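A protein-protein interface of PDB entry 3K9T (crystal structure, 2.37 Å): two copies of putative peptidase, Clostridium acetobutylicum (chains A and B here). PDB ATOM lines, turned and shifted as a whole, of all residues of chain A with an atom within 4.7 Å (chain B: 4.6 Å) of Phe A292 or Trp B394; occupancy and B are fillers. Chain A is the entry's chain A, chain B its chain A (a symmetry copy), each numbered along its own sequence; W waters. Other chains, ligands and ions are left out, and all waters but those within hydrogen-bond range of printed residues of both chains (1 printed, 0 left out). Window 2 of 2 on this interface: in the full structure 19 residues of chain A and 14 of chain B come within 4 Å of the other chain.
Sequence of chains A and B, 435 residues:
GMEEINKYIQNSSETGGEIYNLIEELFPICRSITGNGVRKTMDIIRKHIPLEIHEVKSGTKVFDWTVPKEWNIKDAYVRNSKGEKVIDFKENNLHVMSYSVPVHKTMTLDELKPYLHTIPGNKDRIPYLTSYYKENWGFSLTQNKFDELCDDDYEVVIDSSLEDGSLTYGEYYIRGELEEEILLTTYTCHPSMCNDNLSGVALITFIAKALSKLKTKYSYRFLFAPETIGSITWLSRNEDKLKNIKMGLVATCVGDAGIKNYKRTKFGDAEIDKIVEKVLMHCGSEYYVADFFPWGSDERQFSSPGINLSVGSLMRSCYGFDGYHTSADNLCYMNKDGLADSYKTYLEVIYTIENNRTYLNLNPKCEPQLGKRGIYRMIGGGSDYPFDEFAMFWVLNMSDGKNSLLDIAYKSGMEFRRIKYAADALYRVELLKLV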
ATOM      1  N   LYS A 263     -12.424 -13.794  -4.043  1.00  0.00           N
ATOM      2  CA  LYS A 263     -12.437 -13.883  -5.503  1.00  0.00           C
ATOM      3  C   LYS A 263     -12.781 -15.323  -5.862  1.00  0.00           C
ATOM      4  O   LYS A 263     -12.117 -16.271  -5.444  1.00  0.00           O
ATOM      5  CB  LYS A 263     -11.090 -13.477  -6.103  1.00  0.00           C
ATOM      6  CG  LYS A 263     -10.953 -13.646  -7.611  1.00  0.00           C
ATOM      7  CD  LYS A 263      -9.588 -13.116  -8.073  1.00  0.00           C
ATOM      8  CE  LYS A 263      -9.328 -13.337  -9.565  1.00  0.00           C
ATOM      9  NZ  LYS A 263      -8.073 -12.655 -10.008  1.00  0.00           N
ATOM     10  N   ARG A 264     -13.831 -15.481  -6.642  1.00  0.00           N
ATOM     11  CA  ARG A 264     -14.230 -16.792  -7.067  1.00  0.00           C
ATOM     12  C   ARG A 264     -13.318 -17.448  -8.088  1.00  0.00           C
ATOM     13  O   ARG A 264     -12.596 -16.793  -8.834  1.00  0.00           O
ATOM     14  CB  ARG A 264     -15.597 -16.703  -7.700  1.00  0.00           C
ATOM     15  CG  ARG A 264     -16.652 -16.342  -6.738  1.00  0.00           C
ATOM     16  CD  ARG A 264     -17.874 -16.193  -7.506  1.00  0.00           C
ATOM     17  NE  ARG A 264     -19.020 -16.177  -6.637  1.00  0.00           N
ATOM     18  CZ  ARG A 264     -20.099 -15.446  -6.861  1.00  0.00           C
ATOM     19  NH1 ARG A 264     -20.168 -14.635  -7.907  1.00  0.00           N
ATOM     20  NH2 ARG A 264     -21.106 -15.510  -6.020  1.00  0.00           N
ATOM     21  N   THR A 265     -13.440 -18.763  -8.147  1.00  0.00           N
ATOM     22  CA  THR A 265     -12.860 -19.544  -9.220  1.00  0.00           C
ATOM     23  C   THR A 265     -13.475 -19.113 -10.541  1.00  0.00           C
ATOM     24  O   THR A 265     -14.549 -18.507 -10.560  1.00  0.00           O
ATOM     25  CB  THR A 265     -13.163 -21.059  -9.046  1.00  0.00           C
ATOM     26  OG1 THR A 265     -14.557 -21.347  -9.347  1.00  0.00           O
ATOM     27  CG2 THR A 265     -12.804 -21.499  -7.647  1.00  0.00           C
ATOM     28  N   LYS A 266     -12.820 -19.484 -11.645  1.00  0.00           N
ATOM     29  CA  LYS A 266     -13.314 -19.147 -12.965  1.00  0.00           C
ATOM     30  C   LYS A 266     -14.715 -19.732 -13.184  1.00  0.00           C
ATOM     31  O   LYS A 266     -15.477 -19.186 -13.954  1.00  0.00           O
ATOM     32  CB  LYS A 266     -12.346 -19.591 -14.080  1.00  0.00           C
ATOM     33  CG  LYS A 266     -12.357 -21.110 -14.386  1.00  0.00           C
ATOM     34  CD  LYS A 266     -11.439 -21.553 -15.552  1.00  0.00           C
ATOM     35  CE  LYS A 266     -12.128 -21.761 -16.952  1.00  0.00           C
ATOM     36  NZ  LYS A 266     -11.032 -21.721 -18.051  1.00  0.00           N
ATOM     37  N   ALA A 290     -16.250 -11.265  -5.282  1.00  0.00           N
ATOM     38  CA  ALA A 290     -16.026 -10.803  -6.670  1.00  0.00           C
ATOM     39  C   ALA A 290     -15.984 -11.997  -7.568  1.00  0.00           C
ATOM     40  O   ALA A 290     -15.593 -13.059  -7.145  1.00  0.00           O
ATOM     41  CB  ALA A 290     -14.696 -10.053  -6.785  1.00  0.00           C
ATOM     42  N   ASP A 291     -16.373 -11.828  -8.815  1.00  0.00           N
ATOM     43  CA  ASP A 291     -16.222 -12.893  -9.813  1.00  0.00           C
ATOM     44  C   ASP A 291     -14.777 -12.968 -10.261  1.00  0.00           C
ATOM     45  O   ASP A 291     -13.984 -12.052 -10.073  1.00  0.00           O
ATOM     46  CB  ASP A 291     -17.110 -12.655 -11.052  1.00  0.00           C
ATOM     47  CG  ASP A 291     -18.617 -12.857 -10.768  1.00  0.00           C
ATOM     48  OD1 ASP A 291     -19.025 -13.964 -10.361  1.00  0.00           O
ATOM     49  OD2 ASP A 291     -19.395 -11.892 -10.969  1.00  0.00           O
ATOM     50  N   PHE A 292     -14.443 -14.092 -10.867  1.00  0.00           N
ATOM     51  CA  PHE A 292     -13.129 -14.300 -11.413  1.00  0.00           C
ATOM     52  C   PHE A 292     -12.793 -13.300 -12.489  1.00  0.00           C
ATOM     53  O   PHE A 292     -13.639 -12.862 -13.217  1.00  0.00           O
ATOM     54  CB  PHE A 292     -13.035 -15.686 -12.029  1.00  0.00           C
ATOM     55  CG  PHE A 292     -11.719 -15.964 -12.746  1.00  0.00           C
ATOM     56  CD1 PHE A 292     -10.608 -16.373 -12.042  1.00  0.00           C
ATOM     57  CD2 PHE A 292     -11.630 -15.870 -14.132  1.00  0.00           C
ATOM     58  CE1 PHE A 292      -9.430 -16.663 -12.688  1.00  0.00           C
ATOM     59  CE2 PHE A 292     -10.468 -16.147 -14.779  1.00  0.00           C
ATOM     60  CZ  PHE A 292      -9.354 -16.553 -14.052  1.00  0.00           C
ATOM     61  N   PHE A 293     -11.521 -12.939 -12.543  1.00  0.00           N
ATOM     62  CA  PHE A 293     -10.941 -12.207 -13.662  1.00  0.00           C
ATOM     63  C   PHE A 293      -9.542 -12.782 -13.778  1.00  0.00           C
ATOM     64  O   PHE A 293      -8.925 -13.027 -12.743  1.00  0.00           O
ATOM     65  CB  PHE A 293     -10.920 -10.694 -13.407  1.00  0.00           C
ATOM     66  CG  PHE A 293     -10.437 -10.307 -12.032  1.00  0.00           C
ATOM     67  CD1 PHE A 293     -11.317 -10.246 -10.967  1.00  0.00           C
ATOM     68  CD2 PHE A 293      -9.102  -9.987 -11.812  1.00  0.00           C
ATOM     69  CE1 PHE A 293     -10.867  -9.879  -9.699  1.00  0.00           C
ATOM     70  CE2 PHE A 293      -8.657  -9.613 -10.561  1.00  0.00           C
ATOM     71  CZ  PHE A 293      -9.539  -9.559  -9.507  1.00  0.00           C
ATOM     72  N   PRO A 294      -9.039 -12.982 -15.014  1.00  0.00           N
ATOM     73  CA  PRO A 294      -7.734 -13.585 -15.291  1.00  0.00           C
ATOM     74  C   PRO A 294      -6.510 -12.625 -15.114  1.00  0.00           C
ATOM     75  O   PRO A 294      -5.594 -12.561 -15.946  1.00  0.00           O
ATOM     76  CB  PRO A 294      -7.893 -14.065 -16.727  1.00  0.00           C
ATOM     77  CG  PRO A 294      -8.699 -12.952 -17.339  1.00  0.00           C
ATOM     78  CD  PRO A 294      -9.656 -12.496 -16.252  1.00  0.00           C
ATOM     79  N   TRP A 295      -6.515 -11.885 -14.014  1.00  0.00           N
ATOM     80  CA  TRP A 295      -5.325 -11.179 -13.571  1.00  0.00           C
ATOM     81  C   TRP A 295      -5.398 -11.098 -12.038  1.00  0.00           C
ATOM     82  O   TRP A 295      -6.345 -11.618 -11.431  1.00  0.00           O
ATOM     83  CB  TRP A 295      -5.116  -9.832 -14.289  1.00  0.00           C
ATOM     84  CG  TRP A 295      -6.219  -8.894 -14.099  1.00  0.00           C
ATOM     85  CD1 TRP A 295      -6.377  -8.020 -13.063  1.00  0.00           C
ATOM     86  CD2 TRP A 295      -7.343  -8.720 -14.951  1.00  0.00           C
ATOM     87  NE1 TRP A 295      -7.527  -7.302 -13.226  1.00  0.00           N
ATOM     88  CE2 TRP A 295      -8.148  -7.717 -14.375  1.00  0.00           C
ATOM     89  CE3 TRP A 295      -7.767  -9.329 -16.145  1.00  0.00           C
ATOM     90  CZ2 TRP A 295      -9.358  -7.289 -14.958  1.00  0.00           C
ATOM     91  CZ3 TRP A 295      -8.969  -8.895 -16.736  1.00  0.00           C
ATOM     92  CH2 TRP A 295      -9.741  -7.878 -16.138  1.00  0.00           C
ATOM     93  N   GLU A 299      -4.028 -17.507  -9.275  1.00  0.00           N
ATOM     94  CA  GLU A 299      -5.276 -18.113  -9.749  1.00  0.00           C
ATOM     95  C   GLU A 299      -5.371 -18.017 -11.271  1.00  0.00           C
ATOM     96  O   GLU A 299      -5.996 -18.865 -11.907  1.00  0.00           O
ATOM     97  CB  GLU A 299      -6.489 -17.493  -9.062  1.00  0.00           C
ATOM     98  CG  GLU A 299      -6.742 -16.028  -9.383  1.00  0.00           C
ATOM     99  CD  GLU A 299      -5.938 -15.062  -8.549  1.00  0.00           C
ATOM    100  OE1 GLU A 299      -5.093 -15.523  -7.739  1.00  0.00           O
ATOM    101  OE2 GLU A 299      -6.180 -13.836  -8.713  1.00  0.00           O
ATOM    102  N   SER A 303      -6.070 -21.309 -13.300  1.00  0.00           N
ATOM    103  CA  SER A 303      -7.311 -21.209 -14.052  1.00  0.00           C
ATOM    104  C   SER A 303      -7.119 -21.080 -15.556  1.00  0.00           C
ATOM    105  O   SER A 303      -8.100 -20.865 -16.247  1.00  0.00           O
ATOM    106  CB  SER A 303      -8.091 -20.009 -13.548  1.00  0.00           C
ATOM    107  OG  SER A 303      -8.369 -20.181 -12.167  1.00  0.00           O
ATOM    108  N   PHE B 390      -5.664  -6.454 -20.329  1.00  0.00           N
ATOM    109  CA  PHE B 390      -6.804  -7.082 -19.655  1.00  0.00           C
ATOM    110  C   PHE B 390      -7.683  -7.819 -20.645  1.00  0.00           C
ATOM    111  O   PHE B 390      -8.002  -8.970 -20.427  1.00  0.00           O
ATOM    112  CB  PHE B 390      -7.613  -6.048 -18.885  1.00  0.00           C
ATOM    113  CG  PHE B 390      -6.793  -5.300 -17.911  1.00  0.00           C
ATOM    114  CD1 PHE B 390      -6.472  -5.876 -16.695  1.00  0.00           C
ATOM    115  CD2 PHE B 390      -6.255  -4.053 -18.244  1.00  0.00           C
ATOM    116  CE1 PHE B 390      -5.669  -5.197 -15.787  1.00  0.00           C
ATOM    117  CE2 PHE B 390      -5.451  -3.368 -17.355  1.00  0.00           C
ATOM    118  CZ  PHE B 390      -5.156  -3.942 -16.117  1.00  0.00           C
ATOM    119  N   ALA B 391      -8.056  -7.170 -21.740  1.00  0.00           N
ATOM    120  CA  ALA B 391      -8.793  -7.858 -22.785  1.00  0.00           C
ATOM    121  C   ALA B 391      -8.023  -9.133 -23.246  1.00  0.00           C
ATOM    122  O   ALA B 391      -8.602 -10.218 -23.470  1.00  0.00           O
ATOM    123  CB  ALA B 391      -9.030  -6.907 -24.003  1.00  0.00           C
ATOM    124  N   MET B 392      -6.718  -9.013 -23.412  1.00  0.00           N
ATOM    125  CA  MET B 392      -5.967 -10.156 -23.955  1.00  0.00           C
ATOM    126  C   MET B 392      -6.048 -11.343 -23.030  1.00  0.00           C
ATOM    127  O   MET B 392      -6.265 -12.469 -23.500  1.00  0.00           O
ATOM    128  CB  MET B 392      -4.508  -9.795 -24.230  1.00  0.00           C
ATOM    129  CG  MET B 392      -4.384  -8.883 -25.405  1.00  0.00           C
ATOM    130  SD  MET B 392      -2.590  -8.693 -26.065  1.00  0.00           S
ATOM    131  CE  MET B 392      -1.448  -9.103 -24.533  1.00  0.00           C
ATOM    132  N   PHE B 393      -5.884 -11.086 -21.721  1.00  0.00           N
ATOM    133  CA  PHE B 393      -5.924 -12.146 -20.710  1.00  0.00           C
ATOM    134  C   PHE B 393      -7.264 -12.876 -20.678  1.00  0.00           C
ATOM    135  O   PHE B 393      -7.298 -14.084 -20.442  1.00  0.00           O
ATOM    136  CB  PHE B 393      -5.596 -11.613 -19.318  1.00  0.00           C
ATOM    137  CG  PHE B 393      -4.151 -11.238 -19.128  1.00  0.00           C
ATOM    138  CD1 PHE B 393      -3.137 -12.151 -19.395  1.00  0.00           C
ATOM    139  CD2 PHE B 393      -3.808  -9.990 -18.597  1.00  0.00           C
ATOM    140  CE1 PHE B 393      -1.802 -11.808 -19.190  1.00  0.00           C
ATOM    141  CE2 PHE B 393      -2.481  -9.636 -18.404  1.00  0.00           C
ATOM    142  CZ  PHE B 393      -1.476 -10.557 -18.687  1.00  0.00           C
ATOM    143  N   TRP B 394      -8.358 -12.143 -20.885  1.00  0.00           N
ATOM    144  CA  TRP B 394      -9.681 -12.765 -21.033  1.00  0.00           C
ATOM    145  C   TRP B 394      -9.774 -13.673 -22.247  1.00  0.00           C
ATOM    146  O   TRP B 394     -10.296 -14.789 -22.136  1.00  0.00           O
ATOM    147  CB  TRP B 394     -10.780 -11.728 -21.164  1.00  0.00           C
ATOM    148  CG  TRP B 394     -11.352 -11.276 -19.872  1.00  0.00           C
ATOM    149  CD1 TRP B 394     -11.305 -10.026 -19.359  1.00  0.00           C
ATOM    150  CD2 TRP B 394     -12.037 -12.077 -18.926  1.00  0.00           C
ATOM    151  NE1 TRP B 394     -11.933  -9.988 -18.153  1.00  0.00           N
ATOM    152  CE2 TRP B 394     -12.407 -11.233 -17.861  1.00  0.00           C
ATOM    153  CE3 TRP B 394     -12.368 -13.435 -18.864  1.00  0.00           C
ATOM    154  CZ2 TRP B 394     -13.127 -11.686 -16.754  1.00  0.00           C
ATOM    155  CZ3 TRP B 394     -13.066 -13.901 -17.754  1.00  0.00           C
ATOM    156  CH2 TRP B 394     -13.433 -13.032 -16.706  1.00  0.00           C
ATOM    157  N   VAL B 395      -9.294 -13.186 -23.399  1.00  0.00           N
ATOM    158  CA  VAL B 395      -9.328 -13.964 -24.625  1.00  0.00           C
ATOM    159  C   VAL B 395      -8.514 -15.252 -24.482  1.00  0.00           C
ATOM    160  O   VAL B 395      -8.960 -16.327 -24.869  1.00  0.00           O
ATOM    161  CB  VAL B 395      -8.843 -13.174 -25.829  1.00  0.00           C
ATOM    162  CG1 VAL B 395      -8.654 -14.104 -26.999  1.00  0.00           C
ATOM    163  CG2 VAL B 395      -9.842 -12.097 -26.183  1.00  0.00           C
ATOM    164  N   LEU B 396      -7.337 -15.151 -23.886  1.00  0.00           N
ATOM    165  CA  LEU B 396      -6.509 -16.340 -23.682  1.00  0.00           C
ATOM    166  C   LEU B 396      -7.181 -17.293 -22.720  1.00  0.00           C
ATOM    167  O   LEU B 396      -7.182 -18.512 -22.925  1.00  0.00           O
ATOM    168  CB  LEU B 396      -5.123 -15.967 -23.152  1.00  0.00           C
ATOM    169  CG  LEU B 396      -4.225 -15.245 -24.174  1.00  0.00           C
ATOM    170  CD1 LEU B 396      -3.101 -14.497 -23.504  1.00  0.00           C
ATOM    171  CD2 LEU B 396      -3.672 -16.276 -25.154  1.00  0.00           C
ATOM    172  N   ASN B 397      -7.786 -16.730 -21.690  1.00  0.00           N
ATOM    173  CA  ASN B 397      -8.291 -17.529 -20.618  1.00  0.00           C
ATOM    174  C   ASN B 397      -9.539 -18.289 -21.014  1.00  0.00           C
ATOM    175  O   ASN B 397      -9.696 -19.463 -20.664  1.00  0.00           O
ATOM    176  CB  ASN B 397      -8.510 -16.676 -19.376  1.00  0.00           C
ATOM    177  CG  ASN B 397      -9.167 -17.445 -18.281  1.00  0.00           C
ATOM    178  OD1 ASN B 397     -10.384 -17.521 -18.256  1.00  0.00           O
ATOM    179  ND2 ASN B 397      -8.375 -18.050 -17.382  1.00  0.00           N
ATOM    180  N   MET B 398     -10.403 -17.640 -21.774  1.00  0.00           N
ATOM    181  CA  MET B 398     -11.654 -18.268 -22.177  1.00  0.00           C
ATOM    182  C   MET B 398     -11.655 -18.943 -23.552  1.00  0.00           C
ATOM    183  O   MET B 398     -12.647 -19.545 -23.902  1.00  0.00           O
ATOM    184  CB  MET B 398     -12.780 -17.248 -22.122  1.00  0.00           C
ATOM    185  CG  MET B 398     -13.166 -16.876 -20.687  1.00  0.00           C
ATOM    186  SD  MET B 398     -14.539 -15.525 -20.688  1.00  0.00           S
ATOM    187  CE  MET B 398     -16.054 -16.667 -21.210  1.00  0.00           C
ATOM    188  N   ILE B 408     -17.003 -13.820 -24.496  1.00  0.00           N
ATOM    189  CA  ILE B 408     -15.921 -13.272 -23.699  1.00  0.00           C
ATOM    190  C   ILE B 408     -16.283 -11.812 -23.372  1.00  0.00           C
ATOM    191  O   ILE B 408     -16.133 -11.361 -22.224  1.00  0.00           O
ATOM    192  CB  ILE B 408     -14.551 -13.471 -24.435  1.00  0.00           C
ATOM    193  CG1 ILE B 408     -14.267 -14.972 -24.650  1.00  0.00           C
ATOM    194  CG2 ILE B 408     -13.385 -12.859 -23.672  1.00  0.00           C
ATOM    195  CD1 ILE B 408     -13.210 -15.254 -25.729  1.00  0.00           C
ATOM    196  N   LYS B 411     -18.968 -12.082 -20.550  1.00  0.00           N
ATOM    197  CA  LYS B 411     -18.377 -12.483 -19.239  1.00  0.00           C
ATOM    198  C   LYS B 411     -17.426 -11.407 -18.673  1.00  0.00           C
ATOM    199  O   LYS B 411     -17.459 -11.114 -17.488  1.00  0.00           O
ATOM    200  CB  LYS B 411     -17.664 -13.841 -19.330  1.00  0.00           C
ATOM    201  CG  LYS B 411     -17.116 -14.369 -18.004  1.00  0.00           C
ATOM    202  CD  LYS B 411     -18.009 -15.433 -17.352  1.00  0.00           C
ATOM    203  CE  LYS B 411     -17.450 -16.832 -17.572  1.00  0.00           C
ATOM    204  NZ  LYS B 411     -18.388 -17.897 -17.133  1.00  0.00           N
ATOM    205  N   SER B 412     -16.597 -10.819 -19.524  1.00  0.00           N
ATOM    206  CA  SER B 412     -15.665  -9.773 -19.091  1.00  0.00           C
ATOM    207  C   SER B 412     -16.352  -8.436 -18.784  1.00  0.00           C
ATOM    208  O   SER B 412     -15.763  -7.542 -18.175  1.00  0.00           O
ATOM    209  CB  SER B 412     -14.579  -9.539 -20.182  1.00  0.00           C
ATOM    210  OG  SER B 412     -15.075  -8.886 -21.352  1.00  0.00           O
ATOM    211  N   MET B 414     -16.721  -6.353 -20.959  1.00  0.00           N
ATOM    212  CA  MET B 414     -16.038  -5.391 -21.802  1.00  0.00           C
ATOM    213  C   MET B 414     -16.774  -5.243 -23.120  1.00  0.00           C
ATOM    214  O   MET B 414     -17.532  -6.113 -23.546  1.00  0.00           O
ATOM    215  CB  MET B 414     -14.568  -5.771 -22.032  1.00  0.00           C
ATOM    216  CG  MET B 414     -13.714  -5.849 -20.775  1.00  0.00           C
ATOM    217  SD  MET B 414     -11.952  -6.437 -21.240  1.00  0.00           S
ATOM    218  CE  MET B 414     -10.944  -5.985 -19.690  1.00  0.00           C
HETATM  219  O   HOH W   1     -12.628 -18.794 -17.572  1.00  0.00           O
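O of Ser A303 is in hydrogen-bond range of ND2 of Asn B397 (3.0 Å).
NZ of Lys A263 lies within hydrogen-bond range of O of Phe A293 (2.9 Å).
The side-chain amino group of Lys A263 lies within hydrogen-bond range of the backbone carbonyl oxygen of Trp A295.
The side-chain hydroxyl (OG) of Ser A303 sits at hydrogen-bond distance from the backbone carbonyl oxygen (O) of Glu A299, at 2.7 Å.
Among the printed residues, merely in contact across the chains: Trp A295 with Phe B390, Pro A294 with Trp B394, Trp A295 with Trp B394, Phe A292 with Trp B394, Pro A294 with Phe B393, Lys A266 with Asn B397, Phe A292 with Asn B397, Pro A294 with Asn B397 and Phe A293 with Trp B394.
Phe A292 touches just these residues of chain B: Trp B394 (3.5 Å) and Asn B397 (3.7 Å).
Printed residues of chain A within 4 Å of Trp B394: Phe A292 (3.5 Å), Phe A293 (3.8 Å), Pro A294 (3.4 Å) and Trp A295 (3.5 Å).
Of the printed residues of chain B, Lys A266 touches Asn B397 (3.7 Å).
Of the printed residues of chain B, Pro A294 touches Phe B393, Trp B394 and Asn B397.
Of the printed residues of chain A, Phe B393 touches Pro A294 (3.5 Å).
Of the printed residues of chain A, Phe B390 touches Trp A295.
Of the printed residues of chain B, Trp A295 touches Phe B390 (3.4 Å) and Trp B394 (3.5 Å).
Arg A264 touches none of the printed residues of chain B.
The nearest printed residue of chain A that does not touch Trp B394 is Asp A291 (6.6 Å).
Of the 13 printed residues of chain B, 4 touch a printed residue of chain A.
Printed residues of chain B that touch a printed residue of chain A: Phe B390, Phe B393, Trp B394 and Asn B397.
Along chain B the printed residues that touch a printed residue of chain A span positions 390 to 397.
Among the printed residues, 10 pairs touch across the chains.
No position is printed for both chains.
Of the 10 pairs that touch across the chains among the printed residues, none has its exchanged pair printed and touching as well.
Water W1 bridges the side-chain amide oxygen of Asn B397 (2.7 Å) and the side-chain amino group of Lys A266 (3.4 Å).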
